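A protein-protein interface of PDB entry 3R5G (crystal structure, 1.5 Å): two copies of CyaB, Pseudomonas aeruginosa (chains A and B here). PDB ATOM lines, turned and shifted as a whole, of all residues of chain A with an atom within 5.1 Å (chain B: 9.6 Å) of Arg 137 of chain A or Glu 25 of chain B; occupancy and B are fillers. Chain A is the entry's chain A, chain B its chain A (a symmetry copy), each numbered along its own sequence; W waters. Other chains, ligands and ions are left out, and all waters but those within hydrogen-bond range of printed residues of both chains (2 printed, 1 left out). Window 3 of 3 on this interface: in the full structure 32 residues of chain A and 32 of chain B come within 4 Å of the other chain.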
ATOM      1  N   ARG A   7       4.918 -19.152  -2.277  1.00  0.00           N
ATOM      2  CA  ARG A   7       5.620 -20.168  -1.444  1.00  0.00           C
ATOM      3  C   ARG A   7       6.999 -20.260  -2.022  1.00  0.00           C
ATOM      4  O   ARG A   7       7.127 -20.518  -3.205  1.00  0.00           O
ATOM      5  CB  ARG A   7       4.959 -21.530  -1.575  1.00  0.00           C
ATOM      6  CG  ARG A   7       5.371 -22.494  -0.492  1.00  0.00           C
ATOM      7  CD  ARG A   7       4.153 -23.098   0.214  1.00  0.00           C
ATOM      8  NE  ARG A   7       4.571 -24.195   1.082  1.00  0.00           N
ATOM      9  CZ  ARG A   7       5.312 -25.217   0.659  1.00  0.00           C
ATOM     10  NH1 ARG A   7       5.690 -25.264  -0.614  1.00  0.00           N
ATOM     11  NH2 ARG A   7       5.679 -26.196   1.508  1.00  0.00           N
ATOM     12  N   TYR A 118      10.697 -24.168   2.740  1.00  0.00           N
ATOM     13  CA  TYR A 118       9.655 -23.404   2.049  1.00  0.00           C
ATOM     14  C   TYR A 118       8.796 -22.659   2.962  1.00  0.00           C
ATOM     15  O   TYR A 118       8.283 -23.173   3.958  1.00  0.00           O
ATOM     16  CB  TYR A 118       8.811 -24.426   1.194  1.00  0.00           C
ATOM     17  CG  TYR A 118       9.607 -24.844  -0.033  1.00  0.00           C
ATOM     18  CD1 TYR A 118       9.594 -24.074  -1.245  1.00  0.00           C
ATOM     19  CD2 TYR A 118      10.370 -25.991  -0.049  1.00  0.00           C
ATOM     20  CE1 TYR A 118      10.376 -24.431  -2.374  1.00  0.00           C
ATOM     21  CE2 TYR A 118      11.081 -26.350  -1.181  1.00  0.00           C
ATOM     22  CZ  TYR A 118      11.092 -25.565  -2.318  1.00  0.00           C
ATOM     23  OH  TYR A 118      11.846 -25.964  -3.441  1.00  0.00           O
ATOM     24  N   ILE A 135       5.483 -16.363   6.720  1.00  0.00           N
ATOM     25  CA  ILE A 135       4.881 -17.257   7.721  1.00  0.00           C
ATOM     26  C   ILE A 135       5.093 -18.723   7.319  1.00  0.00           C
ATOM     27  O   ILE A 135       5.350 -19.061   6.144  1.00  0.00           O
ATOM     28  CB  ILE A 135       3.374 -16.936   7.851  1.00  0.00           C
ATOM     29  CG1 ILE A 135       2.637 -17.238   6.540  1.00  0.00           C
ATOM     30  CG2 ILE A 135       3.103 -15.559   8.324  1.00  0.00           C
ATOM     31  CD1 ILE A 135       1.029 -16.989   6.613  1.00  0.00           C
ATOM     32  N   GLY A 136       4.931 -19.656   8.278  1.00  0.00           N
ATOM     33  CA  GLY A 136       4.991 -21.052   7.966  1.00  0.00           C
ATOM     34  C   GLY A 136       5.765 -21.797   9.037  1.00  0.00           C
ATOM     35  O   GLY A 136       6.461 -21.166   9.915  1.00  0.00           O
ATOM     36  N   ARG A 137       5.587 -23.106   9.062  1.00  0.00           N
ATOM     37  CA  ARG A 137       6.352 -23.975   9.977  1.00  0.00           C
ATOM     38  C   ARG A 137       7.860 -23.745   9.969  1.00  0.00           C
ATOM     39  O   ARG A 137       8.503 -23.850  11.011  1.00  0.00           O
ATOM     40  CB  ARG A 137       5.996 -25.435   9.677  1.00  0.00           C
ATOM     41  CG  ARG A 137       6.570 -26.488  10.533  1.00  0.00           C
ATOM     42  CD  ARG A 137       5.917 -27.866  10.084  1.00  0.00           C
ATOM     43  NE  ARG A 137       6.434 -28.430   8.829  1.00  0.00           N
ATOM     44  CZ  ARG A 137       6.727 -29.735   8.652  1.00  0.00           C
ATOM     45  NH1 ARG A 137       6.588 -30.614   9.656  1.00  0.00           N
ATOM     46  NH2 ARG A 137       7.188 -30.177   7.474  1.00  0.00           N
ATOM     47  N   GLU A 138       8.417 -23.446   8.799  1.00  0.00           N
ATOM     48  CA  GLU A 138       9.858 -23.297   8.633  1.00  0.00           C
ATOM     49  C   GLU A 138      10.302 -21.972   9.212  1.00  0.00           C
ATOM     50  O   GLU A 138      11.416 -21.837   9.754  1.00  0.00           O
ATOM     51  CB  GLU A 138      10.211 -23.387   7.152  1.00  0.00           C
ATOM     52  CG  GLU A 138       9.906 -24.766   6.477  1.00  0.00           C
ATOM     53  CD  GLU A 138      10.678 -25.958   6.938  1.00  0.00           C
ATOM     54  OE1 GLU A 138      11.580 -25.900   7.726  1.00  0.00           O
ATOM     55  OE2 GLU A 138      10.280 -27.077   6.511  1.00  0.00           O
ATOM     56  N   VAL A 139       9.412 -20.972   9.216  1.00  0.00           N
ATOM     57  CA  VAL A 139       9.700 -19.770   9.927  1.00  0.00           C
ATOM     58  C   VAL A 139       9.692 -20.020  11.467  1.00  0.00           C
ATOM     59  O   VAL A 139      10.585 -19.574  12.204  1.00  0.00           O
ATOM     60  CB  VAL A 139       8.667 -18.644   9.612  1.00  0.00           C
ATOM     61  CG1 VAL A 139       8.997 -17.384  10.349  1.00  0.00           C
ATOM     62  CG2 VAL A 139       8.503 -18.429   8.137  1.00  0.00           C
ATOM     63  N   ASN A 140       8.695 -20.754  11.943  1.00  0.00           N
ATOM     64  CA  ASN A 140       8.615 -21.015  13.352  1.00  0.00           C
ATOM     65  C   ASN A 140       9.808 -21.875  13.784  1.00  0.00           C
ATOM     66  O   ASN A 140      10.281 -21.631  14.900  1.00  0.00           O
ATOM     67  CB  ASN A 140       7.364 -21.849  13.633  1.00  0.00           C
ATOM     68  CG  ASN A 140       6.107 -21.054  13.430  1.00  0.00           C
ATOM     69  OD1 ASN A 140       6.159 -19.831  13.135  1.00  0.00           O
ATOM     70  ND2 ASN A 140       4.987 -21.711  13.583  1.00  0.00           N
ATOM     71  N   LEU A 141      10.312 -22.731  12.911  1.00  0.00           N
ATOM     72  CA  LEU A 141      11.486 -23.625  13.318  1.00  0.00           C
ATOM     73  C   LEU A 141      12.727 -22.746  13.548  1.00  0.00           C
ATOM     74  O   LEU A 141      13.453 -22.902  14.480  1.00  0.00           O
ATOM     75  CB  LEU A 141      11.704 -24.763  12.359  1.00  0.00           C
ATOM     76  CG  LEU A 141      12.942 -25.637  12.695  1.00  0.00           C
ATOM     77  CD1 LEU A 141      12.786 -26.277  14.087  1.00  0.00           C
ATOM     78  CD2 LEU A 141      13.096 -26.666  11.609  1.00  0.00           C
ATOM     79  N   PHE A 181       6.895 -29.545  17.207  1.00  0.00           N
ATOM     80  CA  PHE A 181       7.641 -30.500  16.404  1.00  0.00           C
ATOM     81  C   PHE A 181       7.683 -31.823  17.154  1.00  0.00           C
ATOM     82  O   PHE A 181       8.120 -31.907  18.294  1.00  0.00           O
ATOM     83  CB  PHE A 181       9.023 -29.972  16.030  1.00  0.00           C
ATOM     84  CG  PHE A 181       8.998 -28.842  14.984  1.00  0.00           C
ATOM     85  CD1 PHE A 181       9.085 -29.132  13.580  1.00  0.00           C
ATOM     86  CD2 PHE A 181       8.917 -27.509  15.402  1.00  0.00           C
ATOM     87  CE1 PHE A 181       9.071 -28.084  12.612  1.00  0.00           C
ATOM     88  CE2 PHE A 181       8.894 -26.440  14.438  1.00  0.00           C
ATOM     89  CZ  PHE A 181       8.968 -26.750  13.047  1.00  0.00           C
ATOM     90  N   ARG A 183       8.957 -34.685  16.075  1.00  0.00           N
ATOM     91  CA  ARG A 183      10.078 -35.532  15.698  1.00  0.00           C
ATOM     92  C   ARG A 183      11.317 -34.733  16.099  1.00  0.00           C
ATOM     93  O   ARG A 183      11.249 -33.461  16.273  1.00  0.00           O
ATOM     94  CB  ARG A 183      10.002 -35.893  14.171  1.00  0.00           C
ATOM     95  CG  ARG A 183       8.686 -36.596  13.751  1.00  0.00           C
ATOM     96  CD  ARG A 183       7.920 -35.961  12.492  1.00  0.00           C
ATOM     97  NE  ARG A 183       8.010 -34.490  12.235  1.00  0.00           N
ATOM     98  CZ  ARG A 183       7.641 -33.510  13.074  1.00  0.00           C
ATOM     99  NH1 ARG A 183       7.182 -33.795  14.257  1.00  0.00           N
ATOM    100  NH2 ARG A 183       7.715 -32.219  12.735  1.00  0.00           N
ATOM    101  N   GLY B  19      -3.445 -23.898  15.769  1.00  0.00           N
ATOM    102  CA  GLY B  19      -3.896 -24.551  14.548  1.00  0.00           C
ATOM    103  C   GLY B  19      -3.461 -23.804  13.288  1.00  0.00           C
ATOM    104  O   GLY B  19      -3.433 -24.387  12.166  1.00  0.00           O
ATOM    105  N   PHE B  20      -3.129 -22.520  13.402  1.00  0.00           N
ATOM    106  CA  PHE B  20      -2.817 -21.735  12.207  1.00  0.00           C
ATOM    107  C   PHE B  20      -1.577 -22.204  11.470  1.00  0.00           C
ATOM    108  O   PHE B  20      -1.542 -22.213  10.265  1.00  0.00           O
ATOM    109  CB  PHE B  20      -2.626 -20.244  12.550  1.00  0.00           C
ATOM    110  CG  PHE B  20      -2.420 -19.413  11.361  1.00  0.00           C
ATOM    111  CD1 PHE B  20      -3.469 -19.093  10.568  1.00  0.00           C
ATOM    112  CD2 PHE B  20      -1.135 -18.979  11.016  1.00  0.00           C
ATOM    113  CE1 PHE B  20      -3.285 -18.339   9.419  1.00  0.00           C
ATOM    114  CE2 PHE B  20      -0.923 -18.219   9.909  1.00  0.00           C
ATOM    115  CZ  PHE B  20      -1.998 -17.875   9.105  1.00  0.00           C
ATOM    116  N   THR B  21      -0.542 -22.574  12.202  1.00  0.00           N
ATOM    117  CA  THR B  21       0.694 -22.953  11.486  1.00  0.00           C
ATOM    118  C   THR B  21       0.457 -24.165  10.570  1.00  0.00           C
ATOM    119  O   THR B  21       0.927 -24.182   9.450  1.00  0.00           O
ATOM    120  CB  THR B  21       1.866 -23.136  12.397  1.00  0.00           C
ATOM    121  OG1 THR B  21       2.090 -21.881  13.080  1.00  0.00           O
ATOM    122  CG2 THR B  21       3.064 -23.536  11.486  1.00  0.00           C
ATOM    123  N   GLU B  22      -0.318 -25.128  11.061  1.00  0.00           N
ATOM    124  CA  GLU B  22      -0.709 -26.347  10.315  1.00  0.00           C
ATOM    125  C   GLU B  22      -1.477 -25.905   9.071  1.00  0.00           C
ATOM    126  O   GLU B  22      -1.149 -26.292   7.918  1.00  0.00           O
ATOM    127  CB  GLU B  22      -1.584 -27.210  11.248  1.00  0.00           C
ATOM    128  CG  GLU B  22      -0.836 -27.711  12.502  1.00  0.00           C
ATOM    129  CD  GLU B  22      -0.893 -26.774  13.796  1.00  0.00           C
ATOM    130  OE1 GLU B  22      -0.755 -25.514  13.750  1.00  0.00           O
ATOM    131  OE2 GLU B  22      -1.024 -27.354  14.903  1.00  0.00           O
ATOM    132  N   LEU B  23      -2.439 -25.021   9.291  1.00  0.00           N
ATOM    133  CA  LEU B  23      -3.241 -24.472   8.192  1.00  0.00           C
ATOM    134  C   LEU B  23      -2.381 -23.775   7.126  1.00  0.00           C
ATOM    135  O   LEU B  23      -2.668 -23.810   5.913  1.00  0.00           O
ATOM    136  CB  LEU B  23      -4.279 -23.508   8.775  1.00  0.00           C
ATOM    137  CG  LEU B  23      -5.306 -22.956   7.774  1.00  0.00           C
ATOM    138  CD1 LEU B  23      -6.440 -24.004   7.446  1.00  0.00           C
ATOM    139  CD2 LEU B  23      -5.871 -21.598   8.216  1.00  0.00           C
ATOM    140  N   SER B  24      -1.310 -23.120   7.564  1.00  0.00           N
ATOM    141  CA  SER B  24      -0.472 -22.402   6.588  1.00  0.00           C
ATOM    142  C   SER B  24       0.333 -23.329   5.665  1.00  0.00           C
ATOM    143  O   SER B  24       0.842 -22.873   4.631  1.00  0.00           O
ATOM    144  CB  SER B  24       0.478 -21.437   7.294  1.00  0.00           C
ATOM    145  OG  SER B  24       1.531 -22.120   7.947  1.00  0.00           O
ATOM    146  N   GLU B  25       0.470 -24.588   6.074  1.00  0.00           N
ATOM    147  CA  GLU B  25       1.137 -25.622   5.288  1.00  0.00           C
ATOM    148  C   GLU B  25       0.158 -26.424   4.376  1.00  0.00           C
ATOM    149  O   GLU B  25       0.558 -27.442   3.821  1.00  0.00           O
ATOM    150  CB  GLU B  25       1.937 -26.577   6.190  1.00  0.00           C
ATOM    151  CG  GLU B  25       3.033 -25.844   7.035  1.00  0.00           C
ATOM    152  CD  GLU B  25       4.109 -25.189   6.167  1.00  0.00           C
ATOM    153  OE1 GLU B  25       4.400 -25.705   5.082  1.00  0.00           O
ATOM    154  OE2 GLU B  25       4.613 -24.112   6.561  1.00  0.00           O
ATOM    155  N   GLU B  26      -1.095 -26.011   4.251  1.00  0.00           N
ATOM    156  CA  GLU B  26      -2.012 -26.778   3.385  1.00  0.00           C
ATOM    157  C   GLU B  26      -3.024 -25.943   2.589  1.00  0.00           C
ATOM    158  O   GLU B  26      -3.660 -26.443   1.650  1.00  0.00           O
ATOM    159  CB  GLU B  26      -2.695 -27.884   4.195  1.00  0.00           C
ATOM    160  CG  GLU B  26      -3.677 -27.368   5.190  1.00  0.00           C
ATOM    161  CD  GLU B  26      -4.257 -28.432   6.112  1.00  0.00           C
ATOM    162  OE1 GLU B  26      -3.491 -29.182   6.769  1.00  0.00           O
ATOM    163  OE2 GLU B  26      -5.505 -28.472   6.229  1.00  0.00           O
ATOM    164  N   LEU B  27      -3.180 -24.680   2.952  1.00  0.00           N
ATOM    165  CA  LEU B  27      -4.007 -23.731   2.193  1.00  0.00           C
ATOM    166  C   LEU B  27      -3.252 -23.123   1.031  1.00  0.00           C
ATOM    167  O   LEU B  27      -2.092 -22.776   1.174  1.00  0.00           O
ATOM    168  CB  LEU B  27      -4.449 -22.578   3.103  1.00  0.00           C
ATOM    169  CG  LEU B  27      -5.817 -22.660   3.739  1.00  0.00           C
ATOM    170  CD1 LEU B  27      -6.141 -21.355   4.421  1.00  0.00           C
ATOM    171  CD2 LEU B  27      -6.861 -22.994   2.655  1.00  0.00           C
ATOM    172  N   GLU B  28      -3.905 -22.961  -0.119  1.00  0.00           N
ATOM    173  CA  GLU B  28      -3.381 -22.100  -1.194  1.00  0.00           C
ATOM    174  C   GLU B  28      -2.942 -20.767  -0.580  1.00  0.00           C
ATOM    175  O   GLU B  28      -3.584 -20.284   0.365  1.00  0.00           O
ATOM    176  CB  GLU B  28      -4.482 -21.851  -2.254  1.00  0.00           C
ATOM    177  CG  GLU B  28      -4.040 -21.895  -3.742  1.00  0.00           C
ATOM    178  CD  GLU B  28      -3.678 -20.501  -4.318  1.00  0.00           C
ATOM    179  OE1 GLU B  28      -2.664 -19.900  -3.844  1.00  0.00           O
ATOM    180  OE2 GLU B  28      -4.401 -20.028  -5.260  1.00  0.00           O
ATOM    181  N   ALA B  29      -1.850 -20.190  -1.080  1.00  0.00           N
ATOM    182  CA  ALA B  29      -1.329 -18.933  -0.543  1.00  0.00           C
ATOM    183  C   ALA B  29      -2.375 -17.804  -0.570  1.00  0.00           C
ATOM    184  O   ALA B  29      -2.396 -16.957   0.330  1.00  0.00           O
ATOM    185  CB  ALA B  29      -0.041 -18.513  -1.262  1.00  0.00           C
ATOM    186  N   LEU B  32      -5.011 -18.522   2.163  1.00  0.00           N
ATOM    187  CA  LEU B  32      -4.294 -18.226   3.449  1.00  0.00           C
ATOM    188  C   LEU B  32      -4.165 -16.727   3.731  1.00  0.00           C
ATOM    189  O   LEU B  32      -4.467 -16.286   4.866  1.00  0.00           O
ATOM    190  CB  LEU B  32      -2.941 -18.952   3.456  1.00  0.00           C
ATOM    191  CG  LEU B  32      -2.013 -18.745   4.666  1.00  0.00           C
ATOM    192  CD1 LEU B  32      -2.664 -19.294   5.936  1.00  0.00           C
ATOM    193  CD2 LEU B  32      -0.641 -19.436   4.442  1.00  0.00           C
ATOM    194  N   ASP B  60       0.193 -14.496  12.733  1.00  0.00           N
ATOM    195  CA  ASP B  60      -1.134 -14.487  13.380  1.00  0.00           C
ATOM    196  C   ASP B  60      -1.047 -13.997  14.810  1.00  0.00           C
ATOM    197  O   ASP B  60      -2.099 -13.843  15.431  1.00  0.00           O
ATOM    198  CB  ASP B  60      -1.712 -15.909  13.428  1.00  0.00           C
ATOM    199  CG  ASP B  60      -0.746 -16.914  14.100  1.00  0.00           C
ATOM    200  OD1 ASP B  60       0.437 -16.958  13.761  1.00  0.00           O
ATOM    201  OD2 ASP B  60      -1.124 -17.653  15.036  1.00  0.00           O
ATOM    202  N   LYS B 106     -10.552 -27.567   9.760  1.00  0.00           N
ATOM    203  CA  LYS B 106      -9.528 -27.895  10.749  1.00  0.00           C
ATOM    204  C   LYS B 106      -9.696 -26.931  11.930  1.00  0.00           C
ATOM    205  O   LYS B 106     -10.076 -25.777  11.757  1.00  0.00           O
ATOM    206  CB  LYS B 106      -8.130 -27.765  10.147  1.00  0.00           C
ATOM    207  CG  LYS B 106      -7.074 -28.635  10.837  1.00  0.00           C
ATOM    208  CD  LYS B 106      -5.652 -28.008  10.787  1.00  0.00           C
ATOM    209  CE  LYS B 106      -5.401 -26.966  11.939  1.00  0.00           C
ATOM    210  NZ  LYS B 106      -5.752 -27.507  13.320  1.00  0.00           N
HETATM  211  O   HOH W   1       6.975 -22.966   6.310  1.00  0.00           O
HETATM  212  O   HOH W   2       6.806 -25.700   4.047  1.00  0.00           O
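Among the printed residues, merely in contact across the chains: Gly 136 of chain A with Glu 25 of chain B, Arg 137 of chain A with Thr 21 of chain B, Gly 136 of chain A with Ser 24 of chain B and Ile 135 of chain A with Leu 32 of chain B.
The guanidinium group (NH2) of Arg 7 of chain A is in salt-bridge range of the side-chain carboxylate (OE1) of Glu 25 of chain B, 3.8 Å away. The backbone NH of Arg 137 of chain A is in hydrogen-bond range of the side-chain carboxylate of Glu 25 of chain B (2.9 Å). OG1 of Thr 21 of chain B sits at hydrogen-bond distance from ND2 of Asn 140 of chain A, 2.9 Å away.
OD1 of Asn 140 of chain A lies close to O of Gly 136 of chain A (3.5 Å). O of Thr 21 of chain B sits at hydrogen-bond distance from OG of Ser 24 of chain B.
No position is printed for both chains. Of the 7 pairs that touch across the chains among the printed residues, none has its exchanged pair printed and touching as well.
Water W2 lies within hydrogen-bond range of the side-chain carboxylate of Glu 25 of chain B (2.6 Å), the guanidinium group of Arg 7 of chain A (2.8 Å) and the backbone carbonyl oxygen of Tyr 118 of chain A (2.9 Å). Water W1 lies within hydrogen-bond range of OE2 of Glu 25 of chain B, O of Tyr 118 of chain A, N of Glu 138 of chain A and N of Arg 137 of chain A.
Hydrophobic or aromatic side chains of chain B that line the printed part of chain A: Leu 32. Hydrophobic or aromatic side chains of chain A that line the printed part of chain B: Ile 135.
Of the printed residues of chain B, Ile 135 of chain A touches Leu 32. Of chain B, only Ser 24 and Glu 25 come within 4 Å of Gly 136 of chain A. Of chain B, only Thr 21 (3.5 Å) and Glu 25 (2.9 Å) come within 4 Å of Arg 137 of chain A. No residue of chain B comes within 4 Å of Glu 138 of chain A. Of chain B, only Thr 21 comes within 4 Å of Asn 140 of chain A. Of the printed residues of chain A, Thr 21 of chain B touches Arg 137 and Asn 140. Of the printed residues of chain A, Glu 25 of chain B touches Arg 7 (3.8 Å), Gly 136 (3.4 Å) and Arg 137 (2.9 Å). Glu 26 of chain B touches none of the printed residues of chain A. Ala 29 of chain B touches none of the printed residues of chain A. Printed residues of chain A within 4 Å of Leu 32 of chain B: Ile 135 (3.7 Å).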
